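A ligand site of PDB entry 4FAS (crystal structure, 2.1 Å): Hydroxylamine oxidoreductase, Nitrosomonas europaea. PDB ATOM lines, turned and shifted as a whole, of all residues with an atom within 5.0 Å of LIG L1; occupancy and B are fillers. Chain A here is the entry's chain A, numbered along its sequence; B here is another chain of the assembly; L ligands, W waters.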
ATOM      1  N   ILE A  56     -11.758   7.919 -13.185  1.00  0.00           N
ATOM      2  CA  ILE A  56     -12.253   8.165 -11.839  1.00  0.00           C
ATOM      3  C   ILE A  56     -12.498   9.643 -11.680  1.00  0.00           C
ATOM      4  O   ILE A  56     -13.253  10.033 -10.814  1.00  0.00           O
ATOM      5  CB  ILE A  56     -11.334   7.677 -10.697  1.00  0.00           C
ATOM      6  CG1 ILE A  56     -10.114   8.569 -10.604  1.00  0.00           C
ATOM      7  CG2 ILE A  56     -11.042   6.202 -10.822  1.00  0.00           C
ATOM      8  CD1 ILE A  56      -9.089   8.208  -9.435  1.00  0.00           C
ATOM      9  N   TYR A  57     -11.794  10.471 -12.458  1.00  0.00           N
ATOM     10  CA  TYR A  57     -11.997  11.959 -12.465  1.00  0.00           C
ATOM     11  C   TYR A  57     -13.087  12.375 -13.419  1.00  0.00           C
ATOM     12  O   TYR A  57     -13.684  13.390 -13.207  1.00  0.00           O
ATOM     13  CB  TYR A  57     -10.674  12.694 -12.776  1.00  0.00           C
ATOM     14  CG  TYR A  57      -9.560  12.379 -11.718  1.00  0.00           C
ATOM     15  CD1 TYR A  57      -9.535  12.988 -10.447  1.00  0.00           C
ATOM     16  CD2 TYR A  57      -8.597  11.415 -12.001  1.00  0.00           C
ATOM     17  CE1 TYR A  57      -8.527  12.677  -9.512  1.00  0.00           C
ATOM     18  CE2 TYR A  57      -7.618  11.073 -11.091  1.00  0.00           C
ATOM     19  CZ  TYR A  57      -7.587  11.711  -9.849  1.00  0.00           C
ATOM     20  OH  TYR A  57      -6.614  11.321  -8.994  1.00  0.00           O
ATOM     21  N   TYR A  64     -15.184   6.774  -8.710  1.00  0.00           N
ATOM     22  CA  TYR A  64     -14.188   7.361  -7.833  1.00  0.00           C
ATOM     23  C   TYR A  64     -14.129   6.707  -6.467  1.00  0.00           C
ATOM     24  O   TYR A  64     -15.133   6.660  -5.775  1.00  0.00           O
ATOM     25  CB  TYR A  64     -14.362   8.887  -7.655  1.00  0.00           C
ATOM     26  CG  TYR A  64     -13.233   9.448  -6.808  1.00  0.00           C
ATOM     27  CD1 TYR A  64     -12.030   9.829  -7.386  1.00  0.00           C
ATOM     28  CD2 TYR A  64     -13.350   9.513  -5.426  1.00  0.00           C
ATOM     29  CE1 TYR A  64     -11.003  10.285  -6.658  1.00  0.00           C
ATOM     30  CE2 TYR A  64     -12.302   9.967  -4.636  1.00  0.00           C
ATOM     31  CZ  TYR A  64     -11.143  10.341  -5.262  1.00  0.00           C
ATOM     32  OH  TYR A  64     -10.109  10.787  -4.516  1.00  0.00           O
ATOM     33  N   LYS A  65     -12.916   6.286  -6.067  1.00  0.00           N
ATOM     34  CA  LYS A  65     -12.637   5.912  -4.689  1.00  0.00           C
ATOM     35  C   LYS A  65     -11.389   6.710  -4.162  1.00  0.00           C
ATOM     36  O   LYS A  65     -10.422   6.907  -4.885  1.00  0.00           O
ATOM     37  CB  LYS A  65     -12.520   4.369  -4.672  1.00  0.00           C
ATOM     38  CG  LYS A  65     -11.233   3.745  -4.172  1.00  0.00           C
ATOM     39  CD  LYS A  65     -10.185   3.213  -5.256  1.00  0.00           C
ATOM     40  CE  LYS A  65      -8.875   2.785  -4.522  1.00  0.00           C
ATOM     41  NZ  LYS A  65      -7.624   2.907  -5.363  1.00  0.00           N
ATOM     42  N   PRO A  67      -7.869   7.751  -2.346  1.00  0.00           N
ATOM     43  CA  PRO A  67      -6.594   7.063  -2.402  1.00  0.00           C
ATOM     44  C   PRO A  67      -6.331   6.228  -1.138  1.00  0.00           C
ATOM     45  O   PRO A  67      -6.858   6.521  -0.055  1.00  0.00           O
ATOM     46  CB  PRO A  67      -5.581   8.196  -2.529  1.00  0.00           C
ATOM     47  CG  PRO A  67      -6.333   9.502  -2.447  1.00  0.00           C
ATOM     48  CD  PRO A  67      -7.722   9.189  -2.037  1.00  0.00           C
ATOM     49  N   SER A  69      -3.453   5.988   0.070  1.00  0.00           N
ATOM     50  CA  SER A  69      -2.520   6.775   0.835  1.00  0.00           C
ATOM     51  C   SER A  69      -2.714   8.252   0.524  1.00  0.00           C
ATOM     52  O   SER A  69      -3.026   8.587  -0.621  1.00  0.00           O
ATOM     53  CB  SER A  69      -1.089   6.329   0.564  1.00  0.00           C
ATOM     54  OG  SER A  69      -0.248   7.150   1.346  1.00  0.00           O
ATOM     55  N   PRO A  70      -2.587   9.120   1.534  1.00  0.00           N
ATOM     56  CA  PRO A  70      -2.200   8.878   2.929  1.00  0.00           C
ATOM     57  C   PRO A  70      -3.316   8.368   3.848  1.00  0.00           C
ATOM     58  O   PRO A  70      -4.521   8.661   3.632  1.00  0.00           O
ATOM     59  CB  PRO A  70      -1.798  10.265   3.418  1.00  0.00           C
ATOM     60  CG  PRO A  70      -2.668  11.214   2.598  1.00  0.00           C
ATOM     61  CD  PRO A  70      -2.871  10.561   1.280  1.00  0.00           C
ATOM     62  N   GLU A  72      -4.563   8.979   6.798  1.00  0.00           N
ATOM     63  CA  GLU A  72      -4.663  10.024   7.784  1.00  0.00           C
ATOM     64  C   GLU A  72      -6.133  10.484   7.973  1.00  0.00           C
ATOM     65  O   GLU A  72      -7.006  10.270   7.126  1.00  0.00           O
ATOM     66  CB  GLU A  72      -3.722  11.174   7.441  1.00  0.00           C
ATOM     67  CG  GLU A  72      -3.358  12.112   8.608  1.00  0.00           C
ATOM     68  CD  GLU A  72      -3.011  11.380   9.974  1.00  0.00           C
ATOM     69  OE1 GLU A  72      -3.909  11.258  10.900  1.00  0.00           O
ATOM     70  OE2 GLU A  72      -1.819  10.947  10.148  1.00  0.00           O
ATOM     71  N   ALA A  74      -8.328  13.931   9.199  1.00  0.00           N
ATOM     72  CA  ALA A  74      -8.066  15.352   9.159  1.00  0.00           C
ATOM     73  C   ALA A  74      -9.274  16.224   9.414  1.00  0.00           C
ATOM     74  O   ALA A  74     -10.388  15.928   8.974  1.00  0.00           O
ATOM     75  CB  ALA A  74      -7.395  15.755   7.798  1.00  0.00           C
ATOM     76  N   GLU A  75      -9.048  17.331  10.102  1.00  0.00           N
ATOM     77  CA  GLU A  75     -10.058  18.391  10.175  1.00  0.00           C
ATOM     78  C   GLU A  75      -9.845  19.494   9.115  1.00  0.00           C
ATOM     79  O   GLU A  75      -8.895  19.429   8.319  1.00  0.00           O
ATOM     80  CB  GLU A  75     -10.091  18.981  11.567  1.00  0.00           C
ATOM     81  CG  GLU A  75     -10.318  17.875  12.575  1.00  0.00           C
ATOM     82  CD  GLU A  75     -10.054  18.309  14.017  1.00  0.00           C
ATOM     83  OE1 GLU A  75      -9.320  19.343  14.269  1.00  0.00           O
ATOM     84  OE2 GLU A  75     -10.601  17.580  14.884  1.00  0.00           O
ATOM     85  N   ASP A  78      -6.456  21.084   8.601  1.00  0.00           N
ATOM     86  CA  ASP A  78      -5.385  20.220   8.161  1.00  0.00           C
ATOM     87  C   ASP A  78      -5.398  20.024   6.626  1.00  0.00           C
ATOM     88  O   ASP A  78      -4.318  19.721   6.026  1.00  0.00           O
ATOM     89  CB  ASP A  78      -5.426  18.826   8.841  1.00  0.00           C
ATOM     90  CG  ASP A  78      -5.583  18.917  10.387  1.00  0.00           C
ATOM     91  OD1 ASP A  78      -4.717  19.539  11.036  1.00  0.00           O
ATOM     92  OD2 ASP A  78      -6.596  18.388  10.905  1.00  0.00           O
ATOM     93  N   CYS A  79      -6.593  20.107   5.993  1.00  0.00           N
ATOM     94  CA  CYS A  79      -6.689  20.039   4.537  1.00  0.00           C
ATOM     95  C   CYS A  79      -5.786  21.125   3.992  1.00  0.00           C
ATOM     96  O   CYS A  79      -4.928  20.860   3.174  1.00  0.00           O
ATOM     97  CB  CYS A  79      -8.141  20.298   4.030  1.00  0.00           C
ATOM     98  SG  CYS A  79      -9.398  19.284   4.845  1.00  0.00           S
ATOM     99  N   CYS A  82      -1.682  20.759   5.036  1.00  0.00           N
ATOM    100  CA  CYS A  82      -0.873  19.732   4.435  1.00  0.00           C
ATOM    101  C   CYS A  82      -0.796  20.012   2.916  1.00  0.00           C
ATOM    102  O   CYS A  82       0.302  19.982   2.312  1.00  0.00           O
ATOM    103  CB  CYS A  82      -1.494  18.397   4.705  1.00  0.00           C
ATOM    104  SG  CYS A  82      -0.478  17.019   4.122  1.00  0.00           S
ATOM    105  N   HIS A  83      -1.962  20.271   2.304  1.00  0.00           N
ATOM    106  CA  HIS A  83      -2.013  20.595   0.863  1.00  0.00           C
ATOM    107  C   HIS A  83      -1.231  21.861   0.481  1.00  0.00           C
ATOM    108  O   HIS A  83      -0.798  22.032  -0.649  1.00  0.00           O
ATOM    109  CB  HIS A  83      -3.441  20.627   0.360  1.00  0.00           C
ATOM    110  CG  HIS A  83      -3.939  19.267   0.147  1.00  0.00           C
ATOM    111  ND1 HIS A  83      -3.739  18.586  -1.023  1.00  0.00           N
ATOM    112  CD2 HIS A  83      -4.484  18.382   1.000  1.00  0.00           C
ATOM    113  CE1 HIS A  83      -4.209  17.367  -0.916  1.00  0.00           C
ATOM    114  NE2 HIS A  83      -4.663  17.219   0.309  1.00  0.00           N
ATOM    115  N   GLU A  86       1.630  19.826  -0.326  1.00  0.00           N
ATOM    116  CA  GLU A  86       1.506  18.712  -1.263  1.00  0.00           C
ATOM    117  C   GLU A  86       0.945  19.156  -2.609  1.00  0.00           C
ATOM    118  O   GLU A  86       1.250  18.544  -3.621  1.00  0.00           O
ATOM    119  CB  GLU A  86       0.557  17.630  -0.746  1.00  0.00           C
ATOM    120  CG  GLU A  86       1.093  16.834   0.386  1.00  0.00           C
ATOM    121  CD  GLU A  86       2.220  15.934  -0.032  1.00  0.00           C
ATOM    122  OE1 GLU A  86       2.193  15.389  -1.179  1.00  0.00           O
ATOM    123  OE2 GLU A  86       3.108  15.752   0.808  1.00  0.00           O
ATOM    124  N   CYS A 145     -11.701  23.171   1.277  1.00  0.00           N
ATOM    125  CA  CYS A 145     -11.443  21.803   0.773  1.00  0.00           C
ATOM    126  C   CYS A 145     -12.435  20.765   1.332  1.00  0.00           C
ATOM    127  O   CYS A 145     -12.994  19.955   0.558  1.00  0.00           O
ATOM    128  CB  CYS A 145      -9.992  21.343   1.034  1.00  0.00           C
ATOM    129  SG  CYS A 145      -8.765  22.701   1.158  1.00  0.00           S
ATOM    130  N   ILE A 146     -12.664  20.825   2.644  1.00  0.00           N
ATOM    131  CA  ILE A 146     -13.480  19.813   3.334  1.00  0.00           C
ATOM    132  C   ILE A 146     -14.930  19.837   2.846  1.00  0.00           C
ATOM    133  O   ILE A 146     -15.612  18.805   2.819  1.00  0.00           O
ATOM    134  CB  ILE A 146     -13.323  19.944   4.901  1.00  0.00           C
ATOM    135  CG1 ILE A 146     -13.743  18.648   5.660  1.00  0.00           C
ATOM    136  CG2 ILE A 146     -13.988  21.199   5.443  1.00  0.00           C
ATOM    137  CD1 ILE A 146     -13.190  18.576   7.108  1.00  0.00           C
ATOM    138  N   HIS A 149     -14.944  18.510  -0.952  1.00  0.00           N
ATOM    139  CA  HIS A 149     -14.383  17.158  -1.060  1.00  0.00           C
ATOM    140  C   HIS A 149     -14.834  16.161   0.014  1.00  0.00           C
ATOM    141  O   HIS A 149     -14.410  15.021  -0.021  1.00  0.00           O
ATOM    142  CB  HIS A 149     -12.870  17.210  -1.086  1.00  0.00           C
ATOM    143  CG  HIS A 149     -12.313  17.737  -2.366  1.00  0.00           C
ATOM    144  ND1 HIS A 149     -12.358  17.029  -3.535  1.00  0.00           N
ATOM    145  CD2 HIS A 149     -11.730  18.919  -2.656  1.00  0.00           C
ATOM    146  CE1 HIS A 149     -11.790  17.743  -4.492  1.00  0.00           C
ATOM    147  NE2 HIS A 149     -11.405  18.896  -3.987  1.00  0.00           N
ATOM    148  N   VAL A 150     -15.657  16.596   0.956  1.00  0.00           N
ATOM    149  CA  VAL A 150     -16.119  15.699   2.019  1.00  0.00           C
ATOM    150  C   VAL A 150     -17.604  15.838   2.231  1.00  0.00           C
ATOM    151  O   VAL A 150     -18.341  14.929   1.913  1.00  0.00           O
ATOM    152  CB  VAL A 150     -15.310  15.836   3.309  1.00  0.00           C
ATOM    153  CG1 VAL A 150     -15.917  15.080   4.388  1.00  0.00           C
ATOM    154  CG2 VAL A 150     -13.852  15.323   3.108  1.00  0.00           C
ATOM    155  N   ALA A 158     -12.280  13.987   8.917  1.00  0.00           N
ATOM    156  CA  ALA A 158     -12.559  13.146   7.767  1.00  0.00           C
ATOM    157  C   ALA A 158     -11.421  12.118   7.664  1.00  0.00           C
ATOM    158  O   ALA A 158     -10.275  12.350   8.057  1.00  0.00           O
ATOM    159  CB  ALA A 158     -12.724  14.015   6.469  1.00  0.00           C
ATOM    160  N   HIS A 160      -9.149  10.324   5.235  1.00  0.00           N
ATOM    161  CA  HIS A 160      -8.676  10.587   3.847  1.00  0.00           C
ATOM    162  C   HIS A 160      -8.919   9.395   2.936  1.00  0.00           C
ATOM    163  O   HIS A 160      -9.154   9.565   1.736  1.00  0.00           O
ATOM    164  CB  HIS A 160      -7.189  10.942   3.863  1.00  0.00           C
ATOM    165  CG  HIS A 160      -6.768  11.877   2.757  1.00  0.00           C
ATOM    166  ND1 HIS A 160      -6.285  11.429   1.544  1.00  0.00           N
ATOM    167  CD2 HIS A 160      -6.663  13.234   2.721  1.00  0.00           C
ATOM    168  CE1 HIS A 160      -5.974  12.466   0.781  1.00  0.00           C
ATOM    169  NE2 HIS A 160      -6.173  13.572   1.478  1.00  0.00           N
ATOM    170  N   ILE A 164     -13.098  11.208   1.200  1.00  0.00           N
ATOM    171  CA  ILE A 164     -12.749  12.129   0.097  1.00  0.00           C
ATOM    172  C   ILE A 164     -13.567  11.821  -1.146  1.00  0.00           C
ATOM    173  O   ILE A 164     -13.641  10.634  -1.571  1.00  0.00           O
ATOM    174  CB  ILE A 164     -11.267  12.108  -0.268  1.00  0.00           C
ATOM    175  CG1 ILE A 164     -10.417  12.490   0.991  1.00  0.00           C
ATOM    176  CG2 ILE A 164     -11.002  13.065  -1.411  1.00  0.00           C
ATOM    177  CD1 ILE A 164     -10.488  13.940   1.425  1.00  0.00           C
ATOM    178  N   ARG A 165     -14.189  12.858  -1.725  1.00  0.00           N
ATOM    179  CA  ARG A 165     -14.893  12.703  -2.983  1.00  0.00           C
ATOM    180  C   ARG A 165     -14.400  13.753  -3.969  1.00  0.00           C
ATOM    181  O   ARG A 165     -13.854  14.773  -3.531  1.00  0.00           O
ATOM    182  CB  ARG A 165     -16.425  12.817  -2.808  1.00  0.00           C
ATOM    183  CG  ARG A 165     -16.877  14.260  -2.635  1.00  0.00           C
ATOM    184  CD  ARG A 165     -18.241  14.436  -2.009  1.00  0.00           C
ATOM    185  NE  ARG A 165     -18.340  15.807  -1.487  1.00  0.00           N
ATOM    186  CZ  ARG A 165     -19.450  16.315  -0.930  1.00  0.00           C
ATOM    187  NH1 ARG A 165     -20.528  15.542  -0.816  1.00  0.00           N
ATOM    188  NH2 ARG A 165     -19.458  17.569  -0.465  1.00  0.00           N
ATOM    189  N   MET A 166     -14.561  13.470  -5.273  1.00  0.00           N
ATOM    190  CA  MET A 166     -14.477  14.497  -6.308  1.00  0.00           C
ATOM    191  C   MET A 166     -15.851  15.131  -6.375  1.00  0.00           C
ATOM    192  O   MET A 166     -16.857  14.436  -6.533  1.00  0.00           O
ATOM    193  CB  MET A 166     -14.127  13.890  -7.668  1.00  0.00           C
ATOM    194  CG  MET A 166     -12.689  13.314  -7.673  1.00  0.00           C
ATOM    195  SD  MET A 166     -11.474  14.634  -7.396  1.00  0.00           S
ATOM    196  CE  MET A 166     -10.623  14.063  -5.935  1.00  0.00           C
ATOM    197  N   SER B 365      -2.769  16.525  -7.751  1.00  0.00           N
ATOM    198  CA  SER B 365      -2.322  15.391  -6.965  1.00  0.00           C
ATOM    199  C   SER B 365      -1.518  14.492  -7.845  1.00  0.00           C
ATOM    200  O   SER B 365      -1.648  14.506  -9.077  1.00  0.00           O
ATOM    201  CB  SER B 365      -3.520  14.598  -6.407  1.00  0.00           C
ATOM    202  OG  SER B 365      -4.248  13.961  -7.423  1.00  0.00           O
ATOM    203  N   GLU B 366      -0.685  13.694  -7.211  1.00  0.00           N
ATOM    204  CA  GLU B 366       0.181  12.736  -7.902  1.00  0.00           C
ATOM    205  C   GLU B 366      -0.598  11.634  -8.611  1.00  0.00           C
ATOM    206  O   GLU B 366      -0.235  11.224  -9.737  1.00  0.00           O
ATOM    207  CB  GLU B 366       1.157  12.057  -6.906  1.00  0.00           C
ATOM    208  CG  GLU B 366       1.922  10.989  -7.576  1.00  0.00           C
ATOM    209  CD  GLU B 366       3.112  10.574  -6.770  1.00  0.00           C
ATOM    210  OE1 GLU B 366       3.221  11.036  -5.602  1.00  0.00           O
ATOM    211  OE2 GLU B 366       3.909   9.755  -7.327  1.00  0.00           O
ATOM    212  N   ARG B 367      -1.663  11.173  -7.976  1.00  0.00           N
ATOM    213  CA  ARG B 367      -2.556  10.203  -8.598  1.00  0.00           C
ATOM    214  C   ARG B 367      -3.189  10.724  -9.897  1.00  0.00           C
ATOM    215  O   ARG B 367      -3.277  10.013 -10.968  1.00  0.00           O
ATOM    216  CB  ARG B 367      -3.595   9.818  -7.575  1.00  0.00           C
ATOM    217  CG  ARG B 367      -4.542   8.683  -7.953  1.00  0.00           C
ATOM    218  CD  ARG B 367      -5.622   8.611  -6.848  1.00  0.00           C
ATOM    219  NE  ARG B 367      -6.448   7.398  -6.871  1.00  0.00           N
ATOM    220  CZ  ARG B 367      -7.654   7.304  -6.280  1.00  0.00           C
ATOM    221  NH1 ARG B 367      -8.198   8.333  -5.619  1.00  0.00           N
ATOM    222  NH2 ARG B 367      -8.304   6.153  -6.305  1.00  0.00           N
ATOM    223  N   PHE B 368      -3.626  11.976  -9.854  1.00  0.00           N
ATOM    224  CA  PHE B 368      -4.169  12.603 -11.094  1.00  0.00           C
ATOM    225  C   PHE B 368      -3.105  12.759 -12.184  1.00  0.00           C
ATOM    226  O   PHE B 368      -3.274  12.302 -13.361  1.00  0.00           O
ATOM    227  CB  PHE B 368      -4.832  13.928 -10.758  1.00  0.00           C
ATOM    228  CG  PHE B 368      -5.409  14.631 -11.932  1.00  0.00           C
ATOM    229  CD1 PHE B 368      -4.598  15.493 -12.742  1.00  0.00           C
ATOM    230  CD2 PHE B 368      -6.784  14.535 -12.208  1.00  0.00           C
ATOM    231  CE1 PHE B 368      -5.132  16.149 -13.879  1.00  0.00           C
ATOM    232  CE2 PHE B 368      -7.345  15.203 -13.365  1.00  0.00           C
ATOM    233  CZ  PHE B 368      -6.503  16.021 -14.198  1.00  0.00           C
HETATM  234 FE1  LIG L   1      -5.345  15.419   0.885  1.00  0.00          FE
HETATM  235  C1  LIG L   1      -4.723  13.944  -2.132  1.00  0.00           C
HETATM  236  C2  LIG L   1      -8.394  16.612  -0.303  1.00  0.00           C
HETATM  237  C3  LIG L   1      -6.130  16.408   4.129  1.00  0.00           C
HETATM  238  C4  LIG L   1      -2.053  14.905   1.958  1.00  0.00           C
HETATM  239  N1  LIG L   1      -6.376  15.253  -0.891  1.00  0.00           N
HETATM  240  C5  LIG L   1      -5.956  14.667  -1.998  1.00  0.00           C
HETATM  241  C6  LIG L   1      -6.922  14.814  -3.029  1.00  0.00           C
HETATM  242  C7  LIG L   1      -7.974  15.559  -2.493  1.00  0.00           C
HETATM  243  C8  LIG L   1      -7.573  15.828  -1.179  1.00  0.00           C
HETATM  244  C9  LIG L   1      -9.253  16.026  -3.138  1.00  0.00           C
HETATM  245  C10 LIG L   1      -6.850  14.204  -4.427  1.00  0.00           C
HETATM  246  C11 LIG L   1      -7.401  12.801  -4.331  1.00  0.00           C
HETATM  247  C12 LIG L   1      -7.276  12.098  -5.635  1.00  0.00           C
HETATM  248  O1  LIG L   1      -7.986  11.123  -5.810  1.00  0.00           O
HETATM  249  O2  LIG L   1      -6.421  12.471  -6.493  1.00  0.00           O
HETATM  250  N2  LIG L   1      -6.947  16.346   1.703  1.00  0.00           N
HETATM  251  C13 LIG L   1      -8.080  16.695   1.117  1.00  0.00           C
HETATM  252  C14 LIG L   1      -8.979  17.155   2.038  1.00  0.00           C
HETATM  253  C15 LIG L   1      -8.335  17.113   3.270  1.00  0.00           C
HETATM  254  C16 LIG L   1      -7.075  16.588   3.028  1.00  0.00           C
HETATM  255  C17 LIG L   1     -10.364  17.654   1.753  1.00  0.00           C
HETATM  256  C18 LIG L   1      -8.887  17.515   4.669  1.00  0.00           C
HETATM  257  C19 LIG L   1     -10.205  16.806   5.033  1.00  0.00           C
HETATM  258  N3  LIG L   1      -4.273  15.624   2.752  1.00  0.00           N
HETATM  259  C20 LIG L   1      -4.768  16.074   3.905  1.00  0.00           C
HETATM  260  C21 LIG L   1      -3.815  15.997   4.918  1.00  0.00           C
HETATM  261  C22 LIG L   1      -2.637  15.606   4.291  1.00  0.00           C
HETATM  262  C23 LIG L   1      -2.963  15.378   2.969  1.00  0.00           C
HETATM  263  C24 LIG L   1      -4.120  16.463   6.316  1.00  0.00           C
HETATM  264  C25 LIG L   1      -1.219  15.438   4.802  1.00  0.00           C
HETATM  265  C26 LIG L   1      -1.086  15.622   6.338  1.00  0.00           C
HETATM  266  N4  LIG L   1      -3.735  14.521   0.099  1.00  0.00           N
HETATM  267  C27 LIG L   1      -2.515  14.473   0.639  1.00  0.00           C
HETATM  268  C28 LIG L   1      -1.639  13.851  -0.269  1.00  0.00           C
HETATM  269  C29 LIG L   1      -2.397  13.536  -1.423  1.00  0.00           C
HETATM  270  C30 LIG L   1      -3.672  14.029  -1.167  1.00  0.00           C
HETATM  271  C31 LIG L   1      -0.160  13.464  -0.029  1.00  0.00           C
HETATM  272  C32 LIG L   1      -1.888  12.903  -2.699  1.00  0.00           C
HETATM  273  C33 LIG L   1      -2.266  11.438  -2.875  1.00  0.00           C
HETATM  274  C34 LIG L   1      -1.928  10.965  -4.296  1.00  0.00           C
HETATM  275  O3  LIG L   1      -1.796   9.748  -4.537  1.00  0.00           O
HETATM  276  O4  LIG L   1      -1.839  11.734  -5.277  1.00  0.00           O
HETATM  277 FE1  LG2 L   2     -10.560  20.528  -5.046  1.00  0.00          FE
HETATM  278  C1  LG2 L   2     -10.218  18.265  -7.641  1.00  0.00           C
HETATM  279  C2  LG2 L   2      -7.512  19.510  -3.760  1.00  0.00           C
HETATM  280  C3  LG2 L   2     -10.874  22.936  -2.511  1.00  0.00           C
HETATM  281  C4  LG2 L   2     -13.732  21.407  -6.227  1.00  0.00           C
HETATM  282  N1  LG2 L   2      -9.135  19.148  -5.595  1.00  0.00           N
HETATM  283  C5  LG2 L   2      -9.170  18.313  -6.675  1.00  0.00           C
HETATM  284  C6  LG2 L   2      -8.008  17.489  -6.706  1.00  0.00           C
HETATM  285  C7  LG2 L   2      -7.219  17.903  -5.651  1.00  0.00           C
HETATM  286  C8  LG2 L   2      -7.961  18.883  -4.973  1.00  0.00           C
HETATM  287  C9  LG2 L   2      -5.888  17.282  -5.249  1.00  0.00           C
HETATM  288  C10 LG2 L   2      -7.591  16.350  -7.684  1.00  0.00           C
HETATM  289  C11 LG2 L   2      -7.508  16.627  -9.179  1.00  0.00           C
HETATM  290  C12 LG2 L   2      -6.466  17.739  -9.385  1.00  0.00           C
HETATM  291  O1  LG2 L   2      -6.598  18.490 -10.380  1.00  0.00           O
HETATM  292  O2  LG2 L   2      -5.491  17.842  -8.601  1.00  0.00           O
HETATM  293  N2  LG2 L   2      -9.385  21.111  -3.461  1.00  0.00           N
HETATM  294  C13 LG2 L   2      -8.249  20.562  -3.083  1.00  0.00           C
HETATM  295  C14 LG2 L   2      -7.776  21.259  -1.942  1.00  0.00           C
HETATM  296  C15 LG2 L   2      -8.711  22.207  -1.651  1.00  0.00           C
HETATM  297  C16 LG2 L   2      -9.688  22.101  -2.580  1.00  0.00           C
HETATM  298  C17 LG2 L   2      -6.491  21.003  -1.163  1.00  0.00           C
HETATM  299  C18 LG2 L   2      -8.684  23.248  -0.562  1.00  0.00           C
HETATM  300  C19 LG2 L   2      -7.416  24.106  -0.769  1.00  0.00           C
HETATM  301  N3  LG2 L   2     -11.990  21.885  -4.477  1.00  0.00           N
HETATM  302  C20 LG2 L   2     -11.984  22.704  -3.412  1.00  0.00           C
HETATM  303  C21 LG2 L   2     -13.216  23.402  -3.294  1.00  0.00           C
HETATM  304  C22 LG2 L   2     -14.018  22.915  -4.289  1.00  0.00           C
HETATM  305  C23 LG2 L   2     -13.227  22.004  -4.999  1.00  0.00           C
HETATM  306  C24 LG2 L   2     -13.602  24.373  -2.178  1.00  0.00           C
HETATM  307  C25 LG2 L   2     -15.497  23.309  -4.597  1.00  0.00           C
HETATM  308  C26 LG2 L   2     -15.767  24.794  -4.713  1.00  0.00           C
HETATM  309  N4  LG2 L   2     -11.762  19.958  -6.652  1.00  0.00           N
HETATM  310  C27 LG2 L   2     -12.953  20.481  -7.008  1.00  0.00           C
HETATM  311  C28 LG2 L   2     -13.411  19.982  -8.238  1.00  0.00           C
HETATM  312  C29 LG2 L   2     -12.379  19.040  -8.650  1.00  0.00           C
HETATM  313  C30 LG2 L   2     -11.400  19.090  -7.613  1.00  0.00           C
HETATM  314  C31 LG2 L   2     -14.700  20.323  -9.023  1.00  0.00           C
HETATM  315  C32 LG2 L   2     -12.356  18.206  -9.936  1.00  0.00           C
HETATM  316  C33 LG2 L   2     -13.159  16.904  -9.724  1.00  0.00           C
HETATM  317  C34 LG2 L   2     -13.025  15.980 -10.902  1.00  0.00           C
HETATM  318  O3  LG2 L   2     -13.734  14.908 -11.055  1.00  0.00           O
HETATM  319  O4  LG2 L   2     -12.220  16.301 -11.790  1.00  0.00           O
HETATM  320  O   HOH W   1      -0.559   8.242  -6.642  1.00  0.00           O
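Pro 67 touches LIG L1. O of Ser 69 touches C33 of LIG L1 (3.7 Å). Pro 70 touches LIG L1. Ala 74 touches LIG L1 (CB to C24, 3.7 Å). Asp 78 touches LIG L1. Glu 86 touches LIG L1 (OE1 to C31, 3.3 Å). O of Cys 145 touches C17 of LIG L1, at 3.7 Å. His 149 touches LIG L1. Ile 164 touches LIG L1. Met 166 touches LIG L1 (CE to C9, 3.7 Å). Hydrophobic or aromatic side chains within 4 Å of LIG L1: Tyr 57, Tyr 64, Pro 67, Pro 70, Ala 74, His 83, His 149, His 160, Ile 164 and Met 166. Of the 28 residues printed, 19 come within 4 Å of LIG L1. The nearest printed residue that does not touch LIG L1 is Ile 146 (4.02 Å).
Water W1 lies within hydrogen-bond range of O3 of LIG L1 (2.9 Å) and N of Arg 367 of chain B (3.4 Å).
NH1 of Arg 367 of chain B lies within salt-bridge range of O1 of LIG L1, 2.8 Å away. An oxygen (O4) of LIG L1 lies within hydrogen-bond range of the backbone NH of Glu 366 of chain B (3.0 Å). O2 of LIG L1 is in hydrogen-bond range of OH of Tyr 57. SG of Cys 145 is covalently linked to C18 of LG2 L2 (1.8 Å). An iron atom (FE1) of LIG L1 is bound by a ring nitrogen (NE2) of His 160. C25 of LIG L1 is bonded to SG of Cys 82. An oxygen (O2) of LIG L1 lies within hydrogen-bond range of the side-chain hydroxyl of Ser 365 of chain B (2.8 Å). An oxygen (O2) of LG2 L2 lies within hydrogen-bond range of the backbone NH (N) of Ser 365 of chain B (3.1 Å). A ring nitrogen (NE2) of His 149 binds an iron atom (FE1) of LG2 L2. An oxygen (O3) of LG2 L2 sits close to the backbone carbonyl oxygen (O) of Tyr 57 (2.6 Å). A ring nitrogen (NE2) of His 83 binds an iron atom (FE1) of LIG L1 (2.0 Å). The side-chain sulfur (SG) of Cys 79 is bonded to a carbon (C18) of LIG L1 (1.8 Å). The side-chain hydroxyl of Tyr 64 lies within hydrogen-bond range of an oxygen (O1) of LIG L1 (2.5 Å). The backbone NH (N) of Arg 367 of chain B sits at hydrogen-bond distance from an oxygen (O4) of LIG L1 (2.8 Å).
The backbone NH (N) of Phe 368 of chain B lies within hydrogen-bond range of the side-chain hydroxyl (OG) of Ser 365 of chain B (3.2 Å). The backbone NH of Ala 158 lies within hydrogen-bond range of the backbone carbonyl oxygen of Ala 74. The side-chain hydroxyl of Tyr 57 is in hydrogen-bond range of the backbone NH of Phe 368 of chain B (3.2 Å). The side-chain carboxylate (OD2) of Asp 78 lies within hydrogen-bond range of the backbone NH (N) of Glu 75, 2.8 Å away. The side-chain hydroxyl (OH) of Tyr 64 sits at hydrogen-bond distance from the guanidinium group (NH1) of Arg 367 of chain B. O of Arg 165 sits at hydrogen-bond distance from ND1 of His 149, 2.7 Å away. N of His 160 is in hydrogen-bond range of O of Glu 72 (2.9 Å). The guanidinium group of Arg 367 of chain B is in hydrogen-bond range of the backbone carbonyl oxygen of Lys 65 (2.7 Å).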
